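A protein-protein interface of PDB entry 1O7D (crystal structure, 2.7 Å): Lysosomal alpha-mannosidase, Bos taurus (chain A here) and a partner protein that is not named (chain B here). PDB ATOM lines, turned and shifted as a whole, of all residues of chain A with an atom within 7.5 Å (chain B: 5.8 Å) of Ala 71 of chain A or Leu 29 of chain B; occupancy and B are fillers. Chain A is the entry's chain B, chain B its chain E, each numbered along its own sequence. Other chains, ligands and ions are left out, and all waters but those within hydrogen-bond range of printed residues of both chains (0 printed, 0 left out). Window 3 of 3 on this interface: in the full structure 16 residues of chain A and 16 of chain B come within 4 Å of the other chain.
N of Gln 68 of chain A lies within hydrogen-bond range of O of Leu 21 of chain B.
The backbone carbonyl oxygen (O) of Ala 71 of chain A is in hydrogen-bond range of the indole nitrogen (NE1) of Trp 122 of chain B, 2.9 Å away.
The backbone NH (N) of Ala 22 of chain B lies within hydrogen-bond range of the backbone carbonyl oxygen (O) of Leu 30 of chain B (2.9 Å).
NE of Arg 23 of chain B sits close to O of Gly 25 of chain B (3.0 Å).
O of Ala 118 of chain B sits at hydrogen-bond distance from N of Leu 29 of chain B (3.1 Å).
Among the printed residues, pairs that only touch across the chains: Glu 70 of chain A with Arg 23 of chain B (3.3 Å), Asn 67 of chain A with Leu 21 of chain B (3.3 Å), Leu 72 of chain A with Trp 122 of chain B (3.5 Å), Ala 71 of chain A with Leu 29 of chain B (3.6 Å), Gly 74 of chain A with Trp 122 of chain B (3.6 Å), Ala 71 of chain A with Leu 21 of chain B (3.8 Å), Gly 74 of chain A with Arg 23 of chain B (3.9 Å), Ala 73 of chain A with Trp 122 of chain B (3.9 Å), Pro 75 of chain A with Arg 23 of chain B (3.9 Å), Leu 72 of chain A with Phe 62 of chain B (3.97 Å) and Ala 71 of chain A with Ala 22 of chain B (3.99 Å).
Of the printed residues of chain B, Ala 71 of chain A touches Leu 21 (3.8 Å), Ala 22 (3.99 Å), Leu 29 (3.6 Å) and Trp 122 (2.9 Å).
Of chain A, only Ala 71 (3.6 Å) comes within 4 Å of Leu 29 of chain B.
Printed residues of chain A within 4 Å of Leu 21 of chain B: Asn 67 (3.3 Å), Gln 68 (3.5 Å) and Ala 71 (3.8 Å).
Of the printed residues of chain B, Gly 74 of chain A touches Arg 23 and Trp 122.
Of the printed residues of chain A, Ala 22 of chain B touches Ala 71.
Ser 119 of chain B touches none of the printed residues of chain A.
The nearest printed residue of chain B that does not touch Ala 71 of chain A is Phe 62 of chain B (4.3 Å).
The nearest residue of chain A that does not touch Leu 29 of chain B is Glu 70 of chain A (5.4 Å).
Of the 17 printed residues of chain B, 6 touch a printed residue of chain A.
Hydrophobic or aromatic side chains of chain B that line the printed part of chain A: Leu 21, Leu 29, Phe 62 and Trp 122.
Along chain B the printed residues that touch a printed residue of chain A span positions 21 to 122.
Among the printed residues, no Asp or Glu carboxylate lies within 4 Å of a Lys or Arg side-chain nitrogen of the other chain.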
ATOM      1  N   VAL A  65       7.310  -1.882   5.865  1.00  0.00           N
ATOM      2  CA  VAL A  65       8.375  -2.815   6.156  1.00  0.00           C
ATOM      3  C   VAL A  65       8.680  -2.722   7.635  1.00  0.00           C
ATOM      4  O   VAL A  65       8.862  -3.725   8.295  1.00  0.00           O
ATOM      5  CB  VAL A  65       9.628  -2.457   5.344  1.00  0.00           C
ATOM      6  CG1 VAL A  65      10.786  -3.321   5.757  1.00  0.00           C
ATOM      7  CG2 VAL A  65       9.338  -2.628   3.852  1.00  0.00           C
ATOM      8  N   CYS A  66       8.720  -1.503   8.156  1.00  0.00           N
ATOM      9  CA  CYS A  66       8.984  -1.282   9.577  1.00  0.00           C
ATOM     10  C   CYS A  66       7.905  -2.001  10.394  1.00  0.00           C
ATOM     11  O   CYS A  66       8.221  -2.741  11.325  1.00  0.00           O
ATOM     12  CB  CYS A  66       8.985   0.231   9.888  1.00  0.00           C
ATOM     13  SG  CYS A  66       9.455   0.786  11.587  1.00  0.00           S
ATOM     14  N   ASN A  67       6.638  -1.793  10.036  1.00  0.00           N
ATOM     15  CA  ASN A  67       5.531  -2.436  10.734  1.00  0.00           C
ATOM     16  C   ASN A  67       5.632  -3.948  10.706  1.00  0.00           C
ATOM     17  O   ASN A  67       5.580  -4.596  11.753  1.00  0.00           O
ATOM     18  CB  ASN A  67       4.191  -2.032  10.122  1.00  0.00           C
ATOM     19  CG  ASN A  67       3.719  -0.689  10.606  1.00  0.00           C
ATOM     20  OD1 ASN A  67       3.823  -0.383  11.796  1.00  0.00           O
ATOM     21  ND2 ASN A  67       3.191   0.120   9.696  1.00  0.00           N
ATOM     22  N   GLN A  68       5.767  -4.513   9.507  1.00  0.00           N
ATOM     23  CA  GLN A  68       5.854  -5.957   9.357  1.00  0.00           C
ATOM     24  C   GLN A  68       6.957  -6.559  10.200  1.00  0.00           C
ATOM     25  O   GLN A  68       6.779  -7.634  10.740  1.00  0.00           O
ATOM     26  CB  GLN A  68       6.093  -6.359   7.906  1.00  0.00           C
ATOM     27  CG  GLN A  68       5.012  -6.006   6.922  1.00  0.00           C
ATOM     28  CD  GLN A  68       5.110  -6.834   5.632  1.00  0.00           C
ATOM     29  OE1 GLN A  68       6.174  -7.359   5.282  1.00  0.00           O
ATOM     30  NE2 GLN A  68       4.000  -6.942   4.920  1.00  0.00           N
ATOM     31  N   LEU A  69       8.100  -5.889  10.317  1.00  0.00           N
ATOM     32  CA  LEU A  69       9.189  -6.457  11.112  1.00  0.00           C
ATOM     33  C   LEU A  69       8.947  -6.417  12.622  1.00  0.00           C
ATOM     34  O   LEU A  69       9.354  -7.327  13.358  1.00  0.00           O
ATOM     35  CB  LEU A  69      10.518  -5.766  10.784  1.00  0.00           C
ATOM     36  CG  LEU A  69      11.239  -6.308   9.552  1.00  0.00           C
ATOM     37  CD1 LEU A  69      12.556  -5.586   9.390  1.00  0.00           C
ATOM     38  CD2 LEU A  69      11.457  -7.801   9.700  1.00  0.00           C
ATOM     39  N   GLU A  70       8.294  -5.352  13.076  1.00  0.00           N
ATOM     40  CA  GLU A  70       7.980  -5.176  14.484  1.00  0.00           C
ATOM     41  C   GLU A  70       6.997  -6.282  14.864  1.00  0.00           C
ATOM     42  O   GLU A  70       7.009  -6.783  15.984  1.00  0.00           O
ATOM     43  CB  GLU A  70       7.349  -3.796  14.680  1.00  0.00           C
ATOM     44  CG  GLU A  70       7.057  -3.385  16.116  1.00  0.00           C
ATOM     45  CD  GLU A  70       6.447  -1.977  16.206  1.00  0.00           C
ATOM     46  OE1 GLU A  70       5.490  -1.682  15.453  1.00  0.00           O
ATOM     47  OE2 GLU A  70       6.918  -1.161  17.033  1.00  0.00           O
ATOM     48  N   ALA A  71       6.160  -6.668  13.905  1.00  0.00           N
ATOM     49  CA  ALA A  71       5.157  -7.702  14.114  1.00  0.00           C
ATOM     50  C   ALA A  71       5.772  -9.088  14.196  1.00  0.00           C
ATOM     51  O   ALA A  71       5.382  -9.903  15.027  1.00  0.00           O
ATOM     52  CB  ALA A  71       4.119  -7.655  12.987  1.00  0.00           C
ATOM     53  N   LEU A  72       6.732  -9.357  13.323  1.00  0.00           N
ATOM     54  CA  LEU A  72       7.405 -10.650  13.302  1.00  0.00           C
ATOM     55  C   LEU A  72       8.330 -10.875  14.520  1.00  0.00           C
ATOM     56  O   LEU A  72       8.489 -12.006  14.977  1.00  0.00           O
ATOM     57  CB  LEU A  72       8.179 -10.798  11.990  1.00  0.00           C
ATOM     58  CG  LEU A  72       7.292 -10.650  10.750  1.00  0.00           C
ATOM     59  CD1 LEU A  72       8.121 -10.774   9.480  1.00  0.00           C
ATOM     60  CD2 LEU A  72       6.205 -11.694  10.790  1.00  0.00           C
ATOM     61  N   ALA A  73       8.934  -9.811  15.048  1.00  0.00           N
ATOM     62  CA  ALA A  73       9.791  -9.945  16.235  1.00  0.00           C
ATOM     63  C   ALA A  73       8.908  -9.771  17.476  1.00  0.00           C
ATOM     64  O   ALA A  73       7.931  -9.017  17.430  1.00  0.00           O
ATOM     65  CB  ALA A  73      10.884  -8.880  16.217  1.00  0.00           C
ATOM     66  N   GLY A  74       9.224 -10.440  18.586  1.00  0.00           N
ATOM     67  CA  GLY A  74       8.365 -10.275  19.758  1.00  0.00           C
ATOM     68  C   GLY A  74       8.982  -9.680  21.020  1.00  0.00           C
ATOM     69  O   GLY A  74       8.928 -10.335  22.072  1.00  0.00           O
ATOM     70  N   PRO A  75       9.538  -8.445  20.974  1.00  0.00           N
ATOM     71  CA  PRO A  75      10.162  -7.811  22.149  1.00  0.00           C
ATOM     72  C   PRO A  75       9.271  -7.765  23.408  1.00  0.00           C
ATOM     73  O   PRO A  75       9.607  -6.963  24.331  1.00  0.00           O
ATOM     74  CB  PRO A  75      10.517  -6.402  21.647  1.00  0.00           C
ATOM     75  CG  PRO A  75      10.727  -6.613  20.170  1.00  0.00           C
ATOM     76  CD  PRO A  75       9.556  -7.523  19.823  1.00  0.00           C
ATOM     77  N   LEU B  21       0.330  -5.472   8.319  1.00  0.00           N
ATOM     78  CA  LEU B  21       0.801  -6.458   9.273  1.00  0.00           C
ATOM     79  C   LEU B  21       1.418  -5.495  10.255  1.00  0.00           C
ATOM     80  O   LEU B  21       2.338  -4.765   9.901  1.00  0.00           O
ATOM     81  CB  LEU B  21       1.864  -7.382   8.677  1.00  0.00           C
ATOM     82  CG  LEU B  21       2.394  -8.439   9.657  1.00  0.00           C
ATOM     83  CD1 LEU B  21       1.221  -9.214  10.261  1.00  0.00           C
ATOM     84  CD2 LEU B  21       3.376  -9.364   8.939  1.00  0.00           C
ATOM     85  N   ALA B  22       0.916  -5.450  11.478  1.00  0.00           N
ATOM     86  CA  ALA B  22       1.467  -4.472  12.394  1.00  0.00           C
ATOM     87  C   ALA B  22       1.423  -4.842  13.852  1.00  0.00           C
ATOM     88  O   ALA B  22       0.801  -5.820  14.246  1.00  0.00           O
ATOM     89  CB  ALA B  22       0.759  -3.138  12.207  1.00  0.00           C
ATOM     90  N   ARG B  23       2.078  -4.025  14.661  1.00  0.00           N
ATOM     91  CA  ARG B  23       2.080  -4.249  16.086  1.00  0.00           C
ATOM     92  C   ARG B  23       1.042  -3.317  16.646  1.00  0.00           C
ATOM     93  O   ARG B  23       1.283  -2.127  16.749  1.00  0.00           O
ATOM     94  CB  ARG B  23       3.435  -3.912  16.687  1.00  0.00           C
ATOM     95  CG  ARG B  23       4.106  -5.069  17.383  1.00  0.00           C
ATOM     96  CD  ARG B  23       3.261  -5.594  18.512  1.00  0.00           C
ATOM     97  NE  ARG B  23       3.948  -6.660  19.229  1.00  0.00           N
ATOM     98  CZ  ARG B  23       5.138  -6.514  19.797  1.00  0.00           C
ATOM     99  NH1 ARG B  23       5.757  -5.336  19.722  1.00  0.00           N
ATOM    100  NH2 ARG B  23       5.709  -7.536  20.431  1.00  0.00           N
ATOM    101  N   TRP B  24      -0.117  -3.846  17.004  1.00  0.00           N
ATOM    102  CA  TRP B  24      -1.166  -3.002  17.573  1.00  0.00           C
ATOM    103  C   TRP B  24      -0.870  -2.802  19.051  1.00  0.00           C
ATOM    104  O   TRP B  24      -1.198  -1.769  19.627  1.00  0.00           O
ATOM    105  CB  TRP B  24      -2.545  -3.653  17.392  1.00  0.00           C
ATOM    106  CG  TRP B  24      -3.687  -2.812  17.887  1.00  0.00           C
ATOM    107  CD1 TRP B  24      -4.365  -2.960  19.060  1.00  0.00           C
ATOM    108  CD2 TRP B  24      -4.289  -1.694  17.215  1.00  0.00           C
ATOM    109  NE1 TRP B  24      -5.352  -2.011  19.159  1.00  0.00           N
ATOM    110  CE2 TRP B  24      -5.327  -1.220  18.041  1.00  0.00           C
ATOM    111  CE3 TRP B  24      -4.050  -1.047  15.993  1.00  0.00           C
ATOM    112  CZ2 TRP B  24      -6.135  -0.125  17.683  1.00  0.00           C
ATOM    113  CZ3 TRP B  24      -4.854   0.041  15.638  1.00  0.00           C
ATOM    114  CH2 TRP B  24      -5.879   0.490  16.480  1.00  0.00           C
ATOM    115  N   GLY B  25      -0.236  -3.798  19.654  1.00  0.00           N
ATOM    116  CA  GLY B  25       0.098  -3.701  21.059  1.00  0.00           C
ATOM    117  C   GLY B  25       1.016  -4.814  21.528  1.00  0.00           C
ATOM    118  O   GLY B  25       1.503  -5.612  20.719  1.00  0.00           O
ATOM    119  N   GLU B  27       0.805  -7.894  22.867  1.00  0.00           N
ATOM    120  CA  GLU B  27       0.591  -9.225  22.293  1.00  0.00           C
ATOM    121  C   GLU B  27      -0.604  -9.132  21.367  1.00  0.00           C
ATOM    122  O   GLU B  27      -1.512  -9.970  21.412  1.00  0.00           O
ATOM    123  CB  GLU B  27       0.305 -10.259  23.387  1.00  0.00           C
ATOM    124  CG  GLU B  27       1.459 -10.476  24.347  1.00  0.00           C
ATOM    125  CD  GLU B  27       1.060 -11.234  25.580  1.00  0.00           C
ATOM    126  OE1 GLU B  27      -0.162 -11.300  25.876  1.00  0.00           O
ATOM    127  OE2 GLU B  27       1.977 -11.749  26.259  1.00  0.00           O
ATOM    128  N   THR B  28      -0.600  -8.103  20.527  1.00  0.00           N
ATOM    129  CA  THR B  28      -1.695  -7.875  19.595  1.00  0.00           C
ATOM    130  C   THR B  28      -1.257  -7.258  18.259  1.00  0.00           C
ATOM    131  O   THR B  28      -0.662  -6.181  18.213  1.00  0.00           O
ATOM    132  CB  THR B  28      -2.777  -6.982  20.251  1.00  0.00           C
ATOM    133  OG1 THR B  28      -3.370  -7.692  21.346  1.00  0.00           O
ATOM    134  CG2 THR B  28      -3.863  -6.616  19.243  1.00  0.00           C
ATOM    135  N   LEU B  29      -1.572  -7.952  17.174  1.00  0.00           N
ATOM    136  CA  LEU B  29      -1.227  -7.488  15.850  1.00  0.00           C
ATOM    137  C   LEU B  29      -2.439  -6.972  15.078  1.00  0.00           C
ATOM    138  O   LEU B  29      -3.565  -7.374  15.338  1.00  0.00           O
ATOM    139  CB  LEU B  29      -0.573  -8.622  15.062  1.00  0.00           C
ATOM    140  CG  LEU B  29       0.772  -9.159  15.569  1.00  0.00           C
ATOM    141  CD1 LEU B  29       1.287 -10.243  14.632  1.00  0.00           C
ATOM    142  CD2 LEU B  29       1.780  -8.028  15.644  1.00  0.00           C
ATOM    143  N   LEU B  30      -2.193  -6.057  14.141  1.00  0.00           N
ATOM    144  CA  LEU B  30      -3.241  -5.510  13.292  1.00  0.00           C
ATOM    145  C   LEU B  30      -3.020  -6.108  11.915  1.00  0.00           C
ATOM    146  O   LEU B  30      -1.933  -6.012  11.359  1.00  0.00           O
ATOM    147  CB  LEU B  30      -3.153  -3.983  13.213  1.00  0.00           C
ATOM    148  CG  LEU B  30      -4.022  -3.331  12.118  1.00  0.00           C
ATOM    149  CD1 LEU B  30      -5.435  -3.851  12.206  1.00  0.00           C
ATOM    150  CD2 LEU B  30      -4.018  -1.822  12.250  1.00  0.00           C
ATOM    151  N   LEU B  31      -4.041  -6.742  11.366  1.00  0.00           N
ATOM    152  CA  LEU B  31      -3.910  -7.343  10.050  1.00  0.00           C
ATOM    153  C   LEU B  31      -5.024  -6.950   9.091  1.00  0.00           C
ATOM    154  O   LEU B  31      -6.192  -6.915   9.459  1.00  0.00           O
ATOM    155  CB  LEU B  31      -3.887  -8.861  10.171  1.00  0.00           C
ATOM    156  CG  LEU B  31      -4.141  -9.602   8.853  1.00  0.00           C
ATOM    157  CD1 LEU B  31      -2.983  -9.364   7.908  1.00  0.00           C
ATOM    158  CD2 LEU B  31      -4.316 -11.093   9.121  1.00  0.00           C
ATOM    159  N   PHE B  62       4.661 -16.382  14.257  1.00  0.00           N
ATOM    160  CA  PHE B  62       3.840 -16.357  15.469  1.00  0.00           C
ATOM    161  C   PHE B  62       2.592 -17.213  15.231  1.00  0.00           C
ATOM    162  O   PHE B  62       2.357 -17.695  14.109  1.00  0.00           O
ATOM    163  CB  PHE B  62       3.427 -14.906  15.775  1.00  0.00           C
ATOM    164  CG  PHE B  62       2.746 -14.224  14.620  1.00  0.00           C
ATOM    165  CD1 PHE B  62       1.379 -14.412  14.379  1.00  0.00           C
ATOM    166  CD2 PHE B  62       3.490 -13.477  13.708  1.00  0.00           C
ATOM    167  CE1 PHE B  62       0.768 -13.879  13.241  1.00  0.00           C
ATOM    168  CE2 PHE B  62       2.884 -12.941  12.567  1.00  0.00           C
ATOM    169  CZ  PHE B  62       1.518 -13.144  12.334  1.00  0.00           C
ATOM    170  N   PHE B 116      -8.553  -7.161  10.909  1.00  0.00           N
ATOM    171  CA  PHE B 116      -8.553  -8.011  12.096  1.00  0.00           C
ATOM    172  C   PHE B 116      -7.587  -7.601  13.184  1.00  0.00           C
ATOM    173  O   PHE B 116      -6.510  -7.083  12.911  1.00  0.00           O
ATOM    174  CB  PHE B 116      -8.217  -9.455  11.714  1.00  0.00           C
ATOM    175  CG  PHE B 116      -9.120 -10.031  10.669  1.00  0.00           C
ATOM    176  CD1 PHE B 116      -8.893  -9.771   9.321  1.00  0.00           C
ATOM    177  CD2 PHE B 116     -10.233 -10.779  11.031  1.00  0.00           C
ATOM    178  CE1 PHE B 116      -9.760 -10.244   8.343  1.00  0.00           C
ATOM    179  CE2 PHE B 116     -11.108 -11.258  10.069  1.00  0.00           C
ATOM    180  CZ  PHE B 116     -10.872 -10.988   8.714  1.00  0.00           C
ATOM    181  N   LEU B 117      -7.996  -7.823  14.426  1.00  0.00           N
ATOM    182  CA  LEU B 117      -7.133  -7.581  15.567  1.00  0.00           C
ATOM    183  C   LEU B 117      -7.022  -8.977  16.142  1.00  0.00           C
ATOM    184  O   LEU B 117      -8.019  -9.552  16.616  1.00  0.00           O
ATOM    185  CB  LEU B 117      -7.759  -6.654  16.602  1.00  0.00           C
ATOM    186  CG  LEU B 117      -7.651  -5.151  16.358  1.00  0.00           C
ATOM    187  CD1 LEU B 117      -7.880  -4.429  17.671  1.00  0.00           C
ATOM    188  CD2 LEU B 117      -6.292  -4.798  15.821  1.00  0.00           C
ATOM    189  N   ALA B 118      -5.822  -9.541  16.067  1.00  0.00           N
ATOM    190  CA  ALA B 118      -5.607 -10.886  16.559  1.00  0.00           C
ATOM    191  C   ALA B 118      -4.536 -10.959  17.627  1.00  0.00           C
ATOM    192  O   ALA B 118      -3.462 -10.396  17.471  1.00  0.00           O
ATOM    193  CB  ALA B 118      -5.248 -11.799  15.415  1.00  0.00           C
ATOM    194  N   SER B 119      -4.852 -11.650  18.719  1.00  0.00           N
ATOM    195  CA  SER B 119      -3.922 -11.837  19.818  1.00  0.00           C
ATOM    196  C   SER B 119      -2.971 -12.916  19.336  1.00  0.00           C
ATOM    197  O   SER B 119      -3.403 -13.900  18.726  1.00  0.00           O
ATOM    198  CB  SER B 119      -4.667 -12.317  21.054  1.00  0.00           C
ATOM    199  OG  SER B 119      -5.754 -11.461  21.328  1.00  0.00           O
ATOM    200  N   VAL B 120      -1.681 -12.741  19.595  1.00  0.00           N
ATOM    201  CA  VAL B 120      -0.719 -13.726  19.129  1.00  0.00           C
ATOM    202  C   VAL B 120       0.279 -14.171  20.163  1.00  0.00           C
ATOM    203  O   VAL B 120       0.330 -13.644  21.278  1.00  0.00           O
ATOM    204  CB  VAL B 120       0.097 -13.203  17.932  1.00  0.00           C
ATOM    205  CG1 VAL B 120      -0.808 -12.953  16.770  1.00  0.00           C
ATOM    206  CG2 VAL B 120       0.848 -11.938  18.320  1.00  0.00           C
ATOM    207  N   TRP B 122       4.517 -15.620  20.020  1.00  0.00           N
ATOM    208  CA  TRP B 122       5.706 -15.873  19.203  1.00  0.00           C
ATOM    209  C   TRP B 122       6.513 -17.154  19.489  1.00  0.00           C
ATOM    210  O   TRP B 122       6.162 -17.909  20.437  1.00  0.00           O
ATOM    211  CB  TRP B 122       6.636 -14.676  19.306  1.00  0.00           C
ATOM    212  CG  TRP B 122       6.139 -13.511  18.576  1.00  0.00           C
ATOM    213  CD1 TRP B 122       6.152 -13.332  17.234  1.00  0.00           C
ATOM    214  CD2 TRP B 122       5.460 -12.391  19.133  1.00  0.00           C
ATOM    215  NE1 TRP B 122       5.512 -12.163  16.904  1.00  0.00           N
ATOM    216  CE2 TRP B 122       5.073 -11.562  18.055  1.00  0.00           C
ATOM    217  CE3 TRP B 122       5.136 -12.007  20.434  1.00  0.00           C
ATOM    218  CZ2 TRP B 122       4.368 -10.358  18.240  1.00  0.00           C
ATOM    219  CZ3 TRP B 122       4.440 -10.817  20.622  1.00  0.00           C
ATOM    220  CH2 TRP B 122       4.061 -10.005  19.523  1.00  0.00           C
